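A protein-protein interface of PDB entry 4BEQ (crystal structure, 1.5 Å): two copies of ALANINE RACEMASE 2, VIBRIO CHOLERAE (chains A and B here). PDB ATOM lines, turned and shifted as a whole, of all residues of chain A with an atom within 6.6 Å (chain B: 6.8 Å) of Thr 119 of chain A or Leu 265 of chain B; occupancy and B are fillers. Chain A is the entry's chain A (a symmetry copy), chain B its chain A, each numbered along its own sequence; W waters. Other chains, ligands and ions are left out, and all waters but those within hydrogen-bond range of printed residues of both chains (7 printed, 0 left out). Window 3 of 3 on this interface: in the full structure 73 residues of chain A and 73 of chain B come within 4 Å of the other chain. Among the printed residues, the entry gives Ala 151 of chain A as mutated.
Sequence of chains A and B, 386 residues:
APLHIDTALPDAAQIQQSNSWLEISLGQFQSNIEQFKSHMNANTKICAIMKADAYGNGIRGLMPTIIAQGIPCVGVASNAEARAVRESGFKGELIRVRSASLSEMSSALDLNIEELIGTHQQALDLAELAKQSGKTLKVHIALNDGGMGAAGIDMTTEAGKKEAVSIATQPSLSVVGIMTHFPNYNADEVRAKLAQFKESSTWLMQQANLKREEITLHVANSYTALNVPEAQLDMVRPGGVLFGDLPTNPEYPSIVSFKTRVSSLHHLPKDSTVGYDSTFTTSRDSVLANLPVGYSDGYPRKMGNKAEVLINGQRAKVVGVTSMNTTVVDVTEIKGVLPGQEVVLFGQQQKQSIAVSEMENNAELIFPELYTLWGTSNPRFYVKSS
Of chain B, only Leu 265 and His 266 come within 4 Å of Thr 119 of chain A. Of the printed residues of chain A, Leu 265 of chain B touches Thr 119. Of the printed residues of chain A, Ser 264 of chain B touches Ser 99 (2.6 Å) and Gln 122 (3.7 Å). Of the printed residues of chain B, Ala 151 of chain A touches His 266 and Asn 290. Of the printed residues of chain B, Ser 99 of chain A touches Ser 263 (2.7 Å), Ser 264 (2.6 Å) and Asn 290 (3.6 Å). Printed residues of chain A within 4 Å of Asn 290 of chain B: Ser 99 (3.6 Å) and Ala 151 (3.7 Å). Of the printed residues of chain A, His 266 of chain B touches Thr 119 (3.5 Å), Ala 151 (3.4 Å) and Gly 152 (3.3 Å). The nearest residue of chain B that does not touch Thr 119 of chain A is Ser 264 of chain B (4.2 Å). The nearest residue of chain A that does not touch Leu 265 of chain B is Glu 163 of chain A (5.2 Å). The nearest printed residue of chain B that does not touch Gly 152 of chain A is Asn 290 of chain B (5.9 Å).
No position is printed for both chains. Of the 9 pairs that touch across the chains among the printed residues, none has its exchanged pair printed and touching as well.
Printed residues of chain B that touch a printed residue of chain A: Ser 263, Ser 264, Leu 265, His 266 and Asn 290. Hydrophobic or aromatic side chains of chain B within 4 Å of the printed part of chain A: His 266. Of the 15 printed residues of chain A, 5 touch a printed residue of chain B. Among the printed residues, 9 pairs touch across the chains. Among the printed residues, no Asp or Glu carboxylate lies within 4 Å of a Lys or Arg side-chain nitrogen of the other chain.
A ring nitrogen (NE2) of His 266 of chain B sits at hydrogen-bond distance from the side-chain hydroxyl of Ser 264 of chain B, at 2.7 Å. O of Ser 264 of chain B is in hydrogen-bond range of N of Asn 290 of chain B, at 2.9 Å. The backbone carbonyl oxygen of His 266 of chain B sits at hydrogen-bond distance from the backbone NH of Leu 288 of chain B (2.8 Å). NE2 of Gln 122 of chain A lies within hydrogen-bond range of OG of Ser 99 of chain A (3.2 Å). N of Gly 118 of chain A sits at hydrogen-bond distance from OE1 of Gln 122 of chain A. The side-chain hydroxyl of Thr 119 of chain A is in hydrogen-bond range of the side-chain amide oxygen of Gln 122 of chain A (2.9 Å).
Water W3 bridges OD1 of Asn 290 of chain B (2.6 Å) and O of Ser 99 of chain A (3.0 Å). Water W2 lies within hydrogen-bond range of the backbone carbonyl oxygen of His 267 of chain B (2.8 Å) and the backbone carbonyl oxygen of Gly 152 of chain A (3.3 Å). Water W7 lies within hydrogen-bond range of O of Gly 118 of chain A (2.8 Å), ND1 of His 266 of chain B (3.0 Å) and O of Gly 152 of chain A (3.2 Å). Water W6 lies within hydrogen-bond range of O of Leu 265 of chain B (2.8 Å) and OE2 of Glu 163 of chain A (2.9 Å). Water W1 lies within hydrogen-bond range of OG1 of Thr 119 of chain A and N of Leu 265 of chain B. Water W4 lies within hydrogen-bond range of OE1 of Glu 163 of chain A (2.9 Å) and N of His 267 of chain B (2.9 Å).
The side-chain hydroxyl of Ser 99 of chain A lies within hydrogen-bond range of the side-chain hydroxyl of Ser 263 of chain B. The side-chain hydroxyl of Ser 264 of chain B is in hydrogen-bond range of the side-chain hydroxyl of Ser 99 of chain A (2.6 Å). O of Gly 152 of chain A is in hydrogen-bond range of ND1 of His 266 of chain B (3.3 Å).
Ser 99 of chain A touches Asn 290 of chain B. Thr 119 of chain A touches Leu 265 of chain B. CG2 of Thr 119 of chain A touches CE1 of His 266 of chain B, at 3.5 Å. CD of Gln 122 of chain A touches CB of Ser 264 of chain B, at 3.7 Å. Ala 151 of chain A touches His 266 of chain B. Ala 151 of chain A touches Asn 290 of chain B (CA to ND2, 3.7 Å).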
ATOM      1  N   SER A  99      -4.115  24.387 -26.037  1.00  0.00           N
ATOM      2  CA  SER A  99      -5.478  24.862 -25.873  1.00  0.00           C
ATOM      3  C   SER A  99      -5.935  25.511 -27.181  1.00  0.00           C
ATOM      4  O   SER A  99      -5.177  26.256 -27.794  1.00  0.00           O
ATOM      5  CB  SER A  99      -5.532  25.888 -24.727  1.00  0.00           C
ATOM      6  OG  SER A  99      -6.859  26.288 -24.509  1.00  0.00           O
ATOM      7  N   ILE A 117      -7.418  19.245 -23.149  1.00  0.00           N
ATOM      8  CA  ILE A 117      -8.190  20.102 -22.267  1.00  0.00           C
ATOM      9  C   ILE A 117      -7.637  20.180 -20.851  1.00  0.00           C
ATOM     10  O   ILE A 117      -7.120  19.192 -20.290  1.00  0.00           O
ATOM     11  CB  ILE A 117      -9.650  19.704 -22.281  1.00  0.00           C
ATOM     12  CG1 ILE A 117      -9.826  18.271 -21.815  1.00  0.00           C
ATOM     13  CG2 ILE A 117     -10.204  19.870 -23.703  1.00  0.00           C
ATOM     14  CD1 ILE A 117     -11.308  17.802 -21.798  1.00  0.00           C
ATOM     15  N   GLY A 118      -7.726  21.372 -20.278  1.00  0.00           N
ATOM     16  CA  GLY A 118      -7.266  21.600 -18.922  1.00  0.00           C
ATOM     17  C   GLY A 118      -8.217  22.400 -18.051  1.00  0.00           C
ATOM     18  O   GLY A 118      -7.841  22.827 -16.968  1.00  0.00           O
ATOM     19  N   THR A 119      -9.445  22.616 -18.519  1.00  0.00           N
ATOM     20  CA  THR A 119     -10.449  23.361 -17.757  1.00  0.00           C
ATOM     21  C   THR A 119     -11.819  22.720 -17.904  1.00  0.00           C
ATOM     22  O   THR A 119     -12.105  22.029 -18.883  1.00  0.00           O
ATOM     23  CB  THR A 119     -10.549  24.847 -18.207  1.00  0.00           C
ATOM     24  OG1 THR A 119     -11.182  24.931 -19.493  1.00  0.00           O
ATOM     25  CG2 THR A 119      -9.187  25.518 -18.268  1.00  0.00           C
ATOM     26  N   HIS A 120     -12.670  22.949 -16.907  1.00  0.00           N
ATOM     27  CA  HIS A 120     -14.029  22.424 -16.941  1.00  0.00           C
ATOM     28  C   HIS A 120     -14.784  22.941 -18.153  1.00  0.00           C
ATOM     29  O   HIS A 120     -15.470  22.189 -18.834  1.00  0.00           O
ATOM     30  CB  HIS A 120     -14.769  22.831 -15.666  1.00  0.00           C
ATOM     31  CG  HIS A 120     -16.033  22.067 -15.444  1.00  0.00           C
ATOM     32  ND1 HIS A 120     -17.027  22.504 -14.596  1.00  0.00           N
ATOM     33  CD2 HIS A 120     -16.467  20.894 -15.959  1.00  0.00           C
ATOM     34  CE1 HIS A 120     -18.018  21.632 -14.599  1.00  0.00           C
ATOM     35  NE2 HIS A 120     -17.704  20.646 -15.419  1.00  0.00           N
ATOM     36  N   GLN A 121     -14.648  24.222 -18.436  1.00  0.00           N
ATOM     37  CA  GLN A 121     -15.384  24.800 -19.551  1.00  0.00           C
ATOM     38  C   GLN A 121     -15.019  24.154 -20.880  1.00  0.00           C
ATOM     39  O   GLN A 121     -15.889  23.918 -21.710  1.00  0.00           O
ATOM     40  CB  GLN A 121     -15.196  26.314 -19.628  1.00  0.00           C
ATOM     41  CG  GLN A 121     -16.165  26.983 -20.596  1.00  0.00           C
ATOM     42  CD  GLN A 121     -17.619  26.765 -20.195  1.00  0.00           C
ATOM     43  OE1 GLN A 121     -18.020  27.091 -19.079  1.00  0.00           O
ATOM     44  NE2 GLN A 121     -18.405  26.203 -21.098  1.00  0.00           N
ATOM     45  N   GLN A 122     -13.740  23.844 -21.092  1.00  0.00           N
ATOM     46  CA  GLN A 122     -13.366  23.128 -22.307  1.00  0.00           C
ATOM     47  C   GLN A 122     -14.060  21.769 -22.370  1.00  0.00           C
ATOM     48  O   GLN A 122     -14.533  21.359 -23.424  1.00  0.00           O
ATOM     49  CB  GLN A 122     -11.850  22.923 -22.408  1.00  0.00           C
ATOM     50  CG  GLN A 122     -11.051  24.172 -22.712  1.00  0.00           C
ATOM     51  CD  GLN A 122      -9.584  23.959 -22.398  1.00  0.00           C
ATOM     52  OE1 GLN A 122      -9.210  23.793 -21.240  1.00  0.00           O
ATOM     53  NE2 GLN A 122      -8.753  23.950 -23.418  1.00  0.00           N
ATOM     54  N   ALA A 123     -14.092  21.053 -21.244  1.00  0.00           N
ATOM     55  CA  ALA A 123     -14.771  19.763 -21.205  1.00  0.00           C
ATOM     56  C   ALA A 123     -16.256  19.897 -21.539  1.00  0.00           C
ATOM     57  O   ALA A 123     -16.793  19.140 -22.346  1.00  0.00           O
ATOM     58  CB  ALA A 123     -14.603  19.126 -19.860  1.00  0.00           C
ATOM     59  N   LEU A 124     -16.904  20.866 -20.912  1.00  0.00           N
ATOM     60  CA  LEU A 124     -18.315  21.148 -21.194  1.00  0.00           C
ATOM     61  C   LEU A 124     -18.569  21.470 -22.665  1.00  0.00           C
ATOM     62  O   LEU A 124     -19.496  20.934 -23.282  1.00  0.00           O
ATOM     63  CB  LEU A 124     -18.793  22.310 -20.328  1.00  0.00           C
ATOM     64  CG  LEU A 124     -18.941  22.011 -18.847  1.00  0.00           C
ATOM     65  CD1 LEU A 124     -19.196  23.277 -18.077  1.00  0.00           C
ATOM     66  CD2 LEU A 124     -20.062  20.993 -18.618  1.00  0.00           C
ATOM     67  N   ALA A 142      -4.774  17.639 -19.880  1.00  0.00           N
ATOM     68  CA  ALA A 142      -3.506  18.241 -19.527  1.00  0.00           C
ATOM     69  C   ALA A 142      -3.469  18.558 -18.026  1.00  0.00           C
ATOM     70  O   ALA A 142      -4.359  19.247 -17.501  1.00  0.00           O
ATOM     71  CB  ALA A 142      -3.284  19.509 -20.348  1.00  0.00           C
ATOM     72  N   ALA A 151      -1.555  25.164 -20.297  1.00  0.00           N
ATOM     73  CA  ALA A 151      -2.696  24.427 -20.833  1.00  0.00           C
ATOM     74  C   ALA A 151      -3.372  23.502 -19.824  1.00  0.00           C
ATOM     75  O   ALA A 151      -4.463  23.014 -20.093  1.00  0.00           O
ATOM     76  CB  ALA A 151      -2.275  23.607 -22.079  1.00  0.00           C
ATOM     77  N   GLY A 152      -2.751  23.272 -18.666  1.00  0.00           N
ATOM     78  CA  GLY A 152      -3.186  22.189 -17.801  1.00  0.00           C
ATOM     79  C   GLY A 152      -4.029  22.594 -16.612  1.00  0.00           C
ATOM     80  O   GLY A 152      -4.194  23.763 -16.298  1.00  0.00           O
ATOM     81  N   ILE A 153      -4.594  21.589 -15.963  1.00  0.00           N
ATOM     82  CA  ILE A 153      -5.307  21.810 -14.726  1.00  0.00           C
ATOM     83  C   ILE A 153      -4.344  21.567 -13.572  1.00  0.00           C
ATOM     84  O   ILE A 153      -3.720  20.508 -13.471  1.00  0.00           O
ATOM     85  CB  ILE A 153      -6.558  20.915 -14.617  1.00  0.00           C
ATOM     86  CG1 ILE A 153      -7.259  21.154 -13.275  1.00  0.00           C
ATOM     87  CG2 ILE A 153      -6.239  19.421 -14.760  1.00  0.00           C
ATOM     88  CD1 ILE A 153      -7.747  22.586 -13.074  1.00  0.00           C
ATOM     89  N   GLU A 163     -11.886  20.241 -10.020  1.00  0.00           N
ATOM     90  CA  GLU A 163     -12.029  20.573 -11.434  1.00  0.00           C
ATOM     91  C   GLU A 163     -11.479  19.447 -12.321  1.00  0.00           C
ATOM     92  O   GLU A 163     -12.100  19.062 -13.316  1.00  0.00           O
ATOM     93  CB  GLU A 163     -11.369  21.921 -11.747  1.00  0.00           C
ATOM     94  CG  GLU A 163     -11.633  22.350 -13.180  1.00  0.00           C
ATOM     95  CD  GLU A 163     -11.242  23.780 -13.492  1.00  0.00           C
ATOM     96  OE1 GLU A 163     -10.736  24.492 -12.597  1.00  0.00           O
ATOM     97  OE2 GLU A 163     -11.459  24.180 -14.663  1.00  0.00           O
ATOM     98  N   ILE A 167     -13.476  17.326 -15.250  1.00  0.00           N
ATOM     99  CA  ILE A 167     -13.016  17.169 -16.626  1.00  0.00           C
ATOM    100  C   ILE A 167     -13.018  15.696 -16.992  1.00  0.00           C
ATOM    101  O   ILE A 167     -13.512  15.284 -18.049  1.00  0.00           O
ATOM    102  CB  ILE A 167     -11.603  17.742 -16.784  1.00  0.00           C
ATOM    103  CG1 ILE A 167     -11.631  19.259 -16.617  1.00  0.00           C
ATOM    104  CG2 ILE A 167     -11.016  17.362 -18.145  1.00  0.00           C
ATOM    105  CD1 ILE A 167     -10.284  19.883 -16.322  1.00  0.00           C
ATOM    106  N   VAL B 262      -9.276  34.617 -26.274  1.00  0.00           N
ATOM    107  CA  VAL B 262      -9.048  33.796 -25.090  1.00  0.00           C
ATOM    108  C   VAL B 262      -9.511  32.378 -25.391  1.00  0.00           C
ATOM    109  O   VAL B 262     -10.684  32.137 -25.683  1.00  0.00           O
ATOM    110  CB  VAL B 262      -9.825  34.353 -23.869  1.00  0.00           C
ATOM    111  CG1 VAL B 262      -9.653  33.446 -22.664  1.00  0.00           C
ATOM    112  CG2 VAL B 262      -9.355  35.755 -23.525  1.00  0.00           C
ATOM    113  N   SER B 263      -8.593  31.432 -25.341  1.00  0.00           N
ATOM    114  CA  SER B 263      -8.986  30.047 -25.538  1.00  0.00           C
ATOM    115  C   SER B 263      -9.573  29.426 -24.286  1.00  0.00           C
ATOM    116  O   SER B 263     -10.632  28.800 -24.328  1.00  0.00           O
ATOM    117  CB  SER B 263      -7.810  29.208 -25.956  1.00  0.00           C
ATOM    118  OG  SER B 263      -8.293  27.898 -26.151  1.00  0.00           O
ATOM    119  N   SER B 264      -8.863  29.599 -23.183  1.00  0.00           N
ATOM    120  CA  SER B 264      -9.247  28.983 -21.929  1.00  0.00           C
ATOM    121  C   SER B 264      -8.791  29.838 -20.742  1.00  0.00           C
ATOM    122  O   SER B 264      -7.875  30.659 -20.869  1.00  0.00           O
ATOM    123  CB  SER B 264      -8.720  27.544 -21.889  1.00  0.00           C
ATOM    124  OG  SER B 264      -7.335  27.469 -22.185  1.00  0.00           O
ATOM    125  N   LEU B 265      -9.475  29.658 -19.606  1.00  0.00           N
ATOM    126  CA  LEU B 265      -9.177  30.384 -18.381  1.00  0.00           C
ATOM    127  C   LEU B 265      -8.802  29.392 -17.279  1.00  0.00           C
ATOM    128  O   LEU B 265      -9.571  28.477 -16.971  1.00  0.00           O
ATOM    129  CB  LEU B 265     -10.388  31.221 -17.934  1.00  0.00           C
ATOM    130  CG  LEU B 265     -10.730  32.405 -18.835  1.00  0.00           C
ATOM    131  CD1 LEU B 265     -12.083  32.987 -18.463  1.00  0.00           C
ATOM    132  CD2 LEU B 265      -9.657  33.467 -18.760  1.00  0.00           C
ATOM    133  N   HIS B 266      -7.634  29.606 -16.683  1.00  0.00           N
ATOM    134  CA  HIS B 266      -7.023  28.660 -15.762  1.00  0.00           C
ATOM    135  C   HIS B 266      -6.790  29.277 -14.384  1.00  0.00           C
ATOM    136  O   HIS B 266      -6.205  30.343 -14.247  1.00  0.00           O
ATOM    137  CB  HIS B 266      -5.688  28.196 -16.333  1.00  0.00           C
ATOM    138  CG  HIS B 266      -5.803  27.598 -17.697  1.00  0.00           C
ATOM    139  ND1 HIS B 266      -5.704  26.242 -17.929  1.00  0.00           N
ATOM    140  CD2 HIS B 266      -6.024  28.163 -18.907  1.00  0.00           C
ATOM    141  CE1 HIS B 266      -5.857  26.003 -19.214  1.00  0.00           C
ATOM    142  NE2 HIS B 266      -6.064  27.154 -19.833  1.00  0.00           N
ATOM    143  N   HIS B 267      -7.227  28.557 -13.357  1.00  0.00           N
ATOM    144  CA  HIS B 267      -6.999  28.966 -11.984  1.00  0.00           C
ATOM    145  C   HIS B 267      -5.673  28.392 -11.503  1.00  0.00           C
ATOM    146  O   HIS B 267      -5.474  27.171 -11.525  1.00  0.00           O
ATOM    147  CB  HIS B 267      -8.172  28.487 -11.128  1.00  0.00           C
ATOM    148  CG  HIS B 267      -9.449  29.202 -11.431  1.00  0.00           C
ATOM    149  ND1 HIS B 267     -10.158  28.997 -12.593  1.00  0.00           N
ATOM    150  CD2 HIS B 267     -10.116  30.161 -10.744  1.00  0.00           C
ATOM    151  CE1 HIS B 267     -11.224  29.781 -12.600  1.00  0.00           C
ATOM    152  NE2 HIS B 267     -11.219  30.496 -11.492  1.00  0.00           N
ATOM    153  N   VAL B 287      -6.058  33.999 -12.021  1.00  0.00           N
ATOM    154  CA  VAL B 287      -6.769  33.438 -13.168  1.00  0.00           C
ATOM    155  C   VAL B 287      -5.983  33.877 -14.400  1.00  0.00           C
ATOM    156  O   VAL B 287      -5.742  35.078 -14.611  1.00  0.00           O
ATOM    157  CB  VAL B 287      -8.208  33.948 -13.269  1.00  0.00           C
ATOM    158  CG1 VAL B 287      -8.897  33.404 -14.520  1.00  0.00           C
ATOM    159  CG2 VAL B 287      -8.992  33.585 -12.009  1.00  0.00           C
ATOM    160  N   LEU B 288      -5.546  32.897 -15.189  1.00  0.00           N
ATOM    161  CA  LEU B 288      -4.704  33.160 -16.350  1.00  0.00           C
ATOM    162  C   LEU B 288      -5.463  32.804 -17.608  1.00  0.00           C
ATOM    163  O   LEU B 288      -6.128  31.756 -17.681  1.00  0.00           O
ATOM    164  CB  LEU B 288      -3.415  32.347 -16.273  1.00  0.00           C
ATOM    165  CG  LEU B 288      -2.593  32.559 -14.995  1.00  0.00           C
ATOM    166  CD1 LEU B 288      -1.326  31.707 -15.054  1.00  0.00           C
ATOM    167  CD2 LEU B 288      -2.247  34.026 -14.805  1.00  0.00           C
ATOM    168  N   ALA B 289      -5.362  33.681 -18.606  1.00  0.00           N
ATOM    169  CA  ALA B 289      -5.950  33.421 -19.910  1.00  0.00           C
ATOM    170  C   ALA B 289      -4.897  32.836 -20.842  1.00  0.00           C
ATOM    171  O   ALA B 289      -3.820  33.390 -20.994  1.00  0.00           O
ATOM    172  CB  ALA B 289      -6.509  34.690 -20.490  1.00  0.00           C
ATOM    173  N   ASN B 290      -5.241  31.711 -21.454  1.00  0.00           N
ATOM    174  CA  ASN B 290      -4.404  31.022 -22.417  1.00  0.00           C
ATOM    175  C   ASN B 290      -4.810  31.481 -23.819  1.00  0.00           C
ATOM    176  O   ASN B 290      -5.959  31.310 -24.231  1.00  0.00           O
ATOM    177  CB  ASN B 290      -4.604  29.507 -22.225  1.00  0.00           C
ATOM    178  CG  ASN B 290      -3.809  28.677 -23.199  1.00  0.00           C
ATOM    179  OD1 ASN B 290      -3.783  28.970 -24.392  1.00  0.00           O
ATOM    180  ND2 ASN B 290      -3.164  27.622 -22.702  1.00  0.00           N
ATOM    181  N   VAL B 329      -1.680  35.249 -20.178  1.00  0.00           N
ATOM    182  CA  VAL B 329      -1.978  36.605 -19.720  1.00  0.00           C
ATOM    183  C   VAL B 329      -2.674  36.561 -18.357  1.00  0.00           C
ATOM    184  O   VAL B 329      -3.497  35.677 -18.095  1.00  0.00           O
ATOM    185  CB  VAL B 329      -2.856  37.319 -20.753  1.00  0.00           C
ATOM    186  CG1 VAL B 329      -3.306  38.706 -20.269  1.00  0.00           C
ATOM    187  CG2 VAL B 329      -2.111  37.409 -22.064  1.00  0.00           C
ATOM    188  N   VAL B 331      -5.314  37.660 -15.981  1.00  0.00           N
ATOM    189  CA  VAL B 331      -6.615  38.340 -15.987  1.00  0.00           C
ATOM    190  C   VAL B 331      -7.266  38.321 -14.601  1.00  0.00           C
ATOM    191  O   VAL B 331      -8.473  38.501 -14.473  1.00  0.00           O
ATOM    192  CB  VAL B 331      -7.579  37.734 -17.044  1.00  0.00           C
ATOM    193  CG1 VAL B 331      -7.010  37.943 -18.437  1.00  0.00           C
ATOM    194  CG2 VAL B 331      -7.840  36.264 -16.804  1.00  0.00           C
ATOM    195  N   VAL B 337     -14.016  38.784 -17.978  1.00  0.00           N
ATOM    196  CA  VAL B 337     -13.304  37.975 -18.984  1.00  0.00           C
ATOM    197  C   VAL B 337     -13.892  36.567 -19.156  1.00  0.00           C
ATOM    198  O   VAL B 337     -14.181  35.873 -18.185  1.00  0.00           O
ATOM    199  CB  VAL B 337     -11.789  37.874 -18.681  1.00  0.00           C
ATOM    200  CG1 VAL B 337     -11.056  37.078 -19.766  1.00  0.00           C
ATOM    201  CG2 VAL B 337     -11.190  39.262 -18.549  1.00  0.00           C
ATOM    202  N   LEU B 338     -14.064  36.162 -20.407  1.00  0.00           N
ATOM    203  CA  LEU B 338     -14.683  34.892 -20.757  1.00  0.00           C
ATOM    204  C   LEU B 338     -13.945  34.278 -21.938  1.00  0.00           C
ATOM    205  O   LEU B 338     -13.391  35.005 -22.775  1.00  0.00           O
ATOM    206  CB  LEU B 338     -16.146  35.094 -21.164  1.00  0.00           C
ATOM    207  CG  LEU B 338     -17.131  35.603 -20.102  1.00  0.00           C
ATOM    208  CD1 LEU B 338     -18.472  35.891 -20.760  1.00  0.00           C
ATOM    209  CD2 LEU B 338     -17.292  34.593 -18.976  1.00  0.00           C
ATOM    210  N   PRO B 339     -13.964  32.941 -22.043  1.00  0.00           N
ATOM    211  CA  PRO B 339     -13.377  32.320 -23.231  1.00  0.00           C
ATOM    212  C   PRO B 339     -14.047  32.848 -24.493  1.00  0.00           C
ATOM    213  O   PRO B 339     -15.256  33.134 -24.512  1.00  0.00           O
ATOM    214  CB  PRO B 339     -13.685  30.834 -23.043  1.00  0.00           C
ATOM    215  CG  PRO B 339     -13.870  30.674 -21.568  1.00  0.00           C
ATOM    216  CD  PRO B 339     -14.534  31.933 -21.125  1.00  0.00           C
HETATM  217  O   HOH W   1     -11.718  27.678 -20.035  1.00  0.00           O
HETATM  218  O   HOH W   2      -4.918  25.316 -13.525  1.00  0.00           O
HETATM  219  O   HOH W   3      -2.930  27.896 -26.646  1.00  0.00           O
HETATM  220  O   HOH W   4      -8.742  26.171 -13.762  1.00  0.00           O
HETATM  221  O   HOH W   5      -1.839  25.717 -24.561  1.00  0.00           O
HETATM  222  O   HOH W   6     -11.270  26.982 -15.254  1.00  0.00           O
HETATM  223  O   HOH W   7      -6.948  25.071 -15.479  1.00  0.00           O
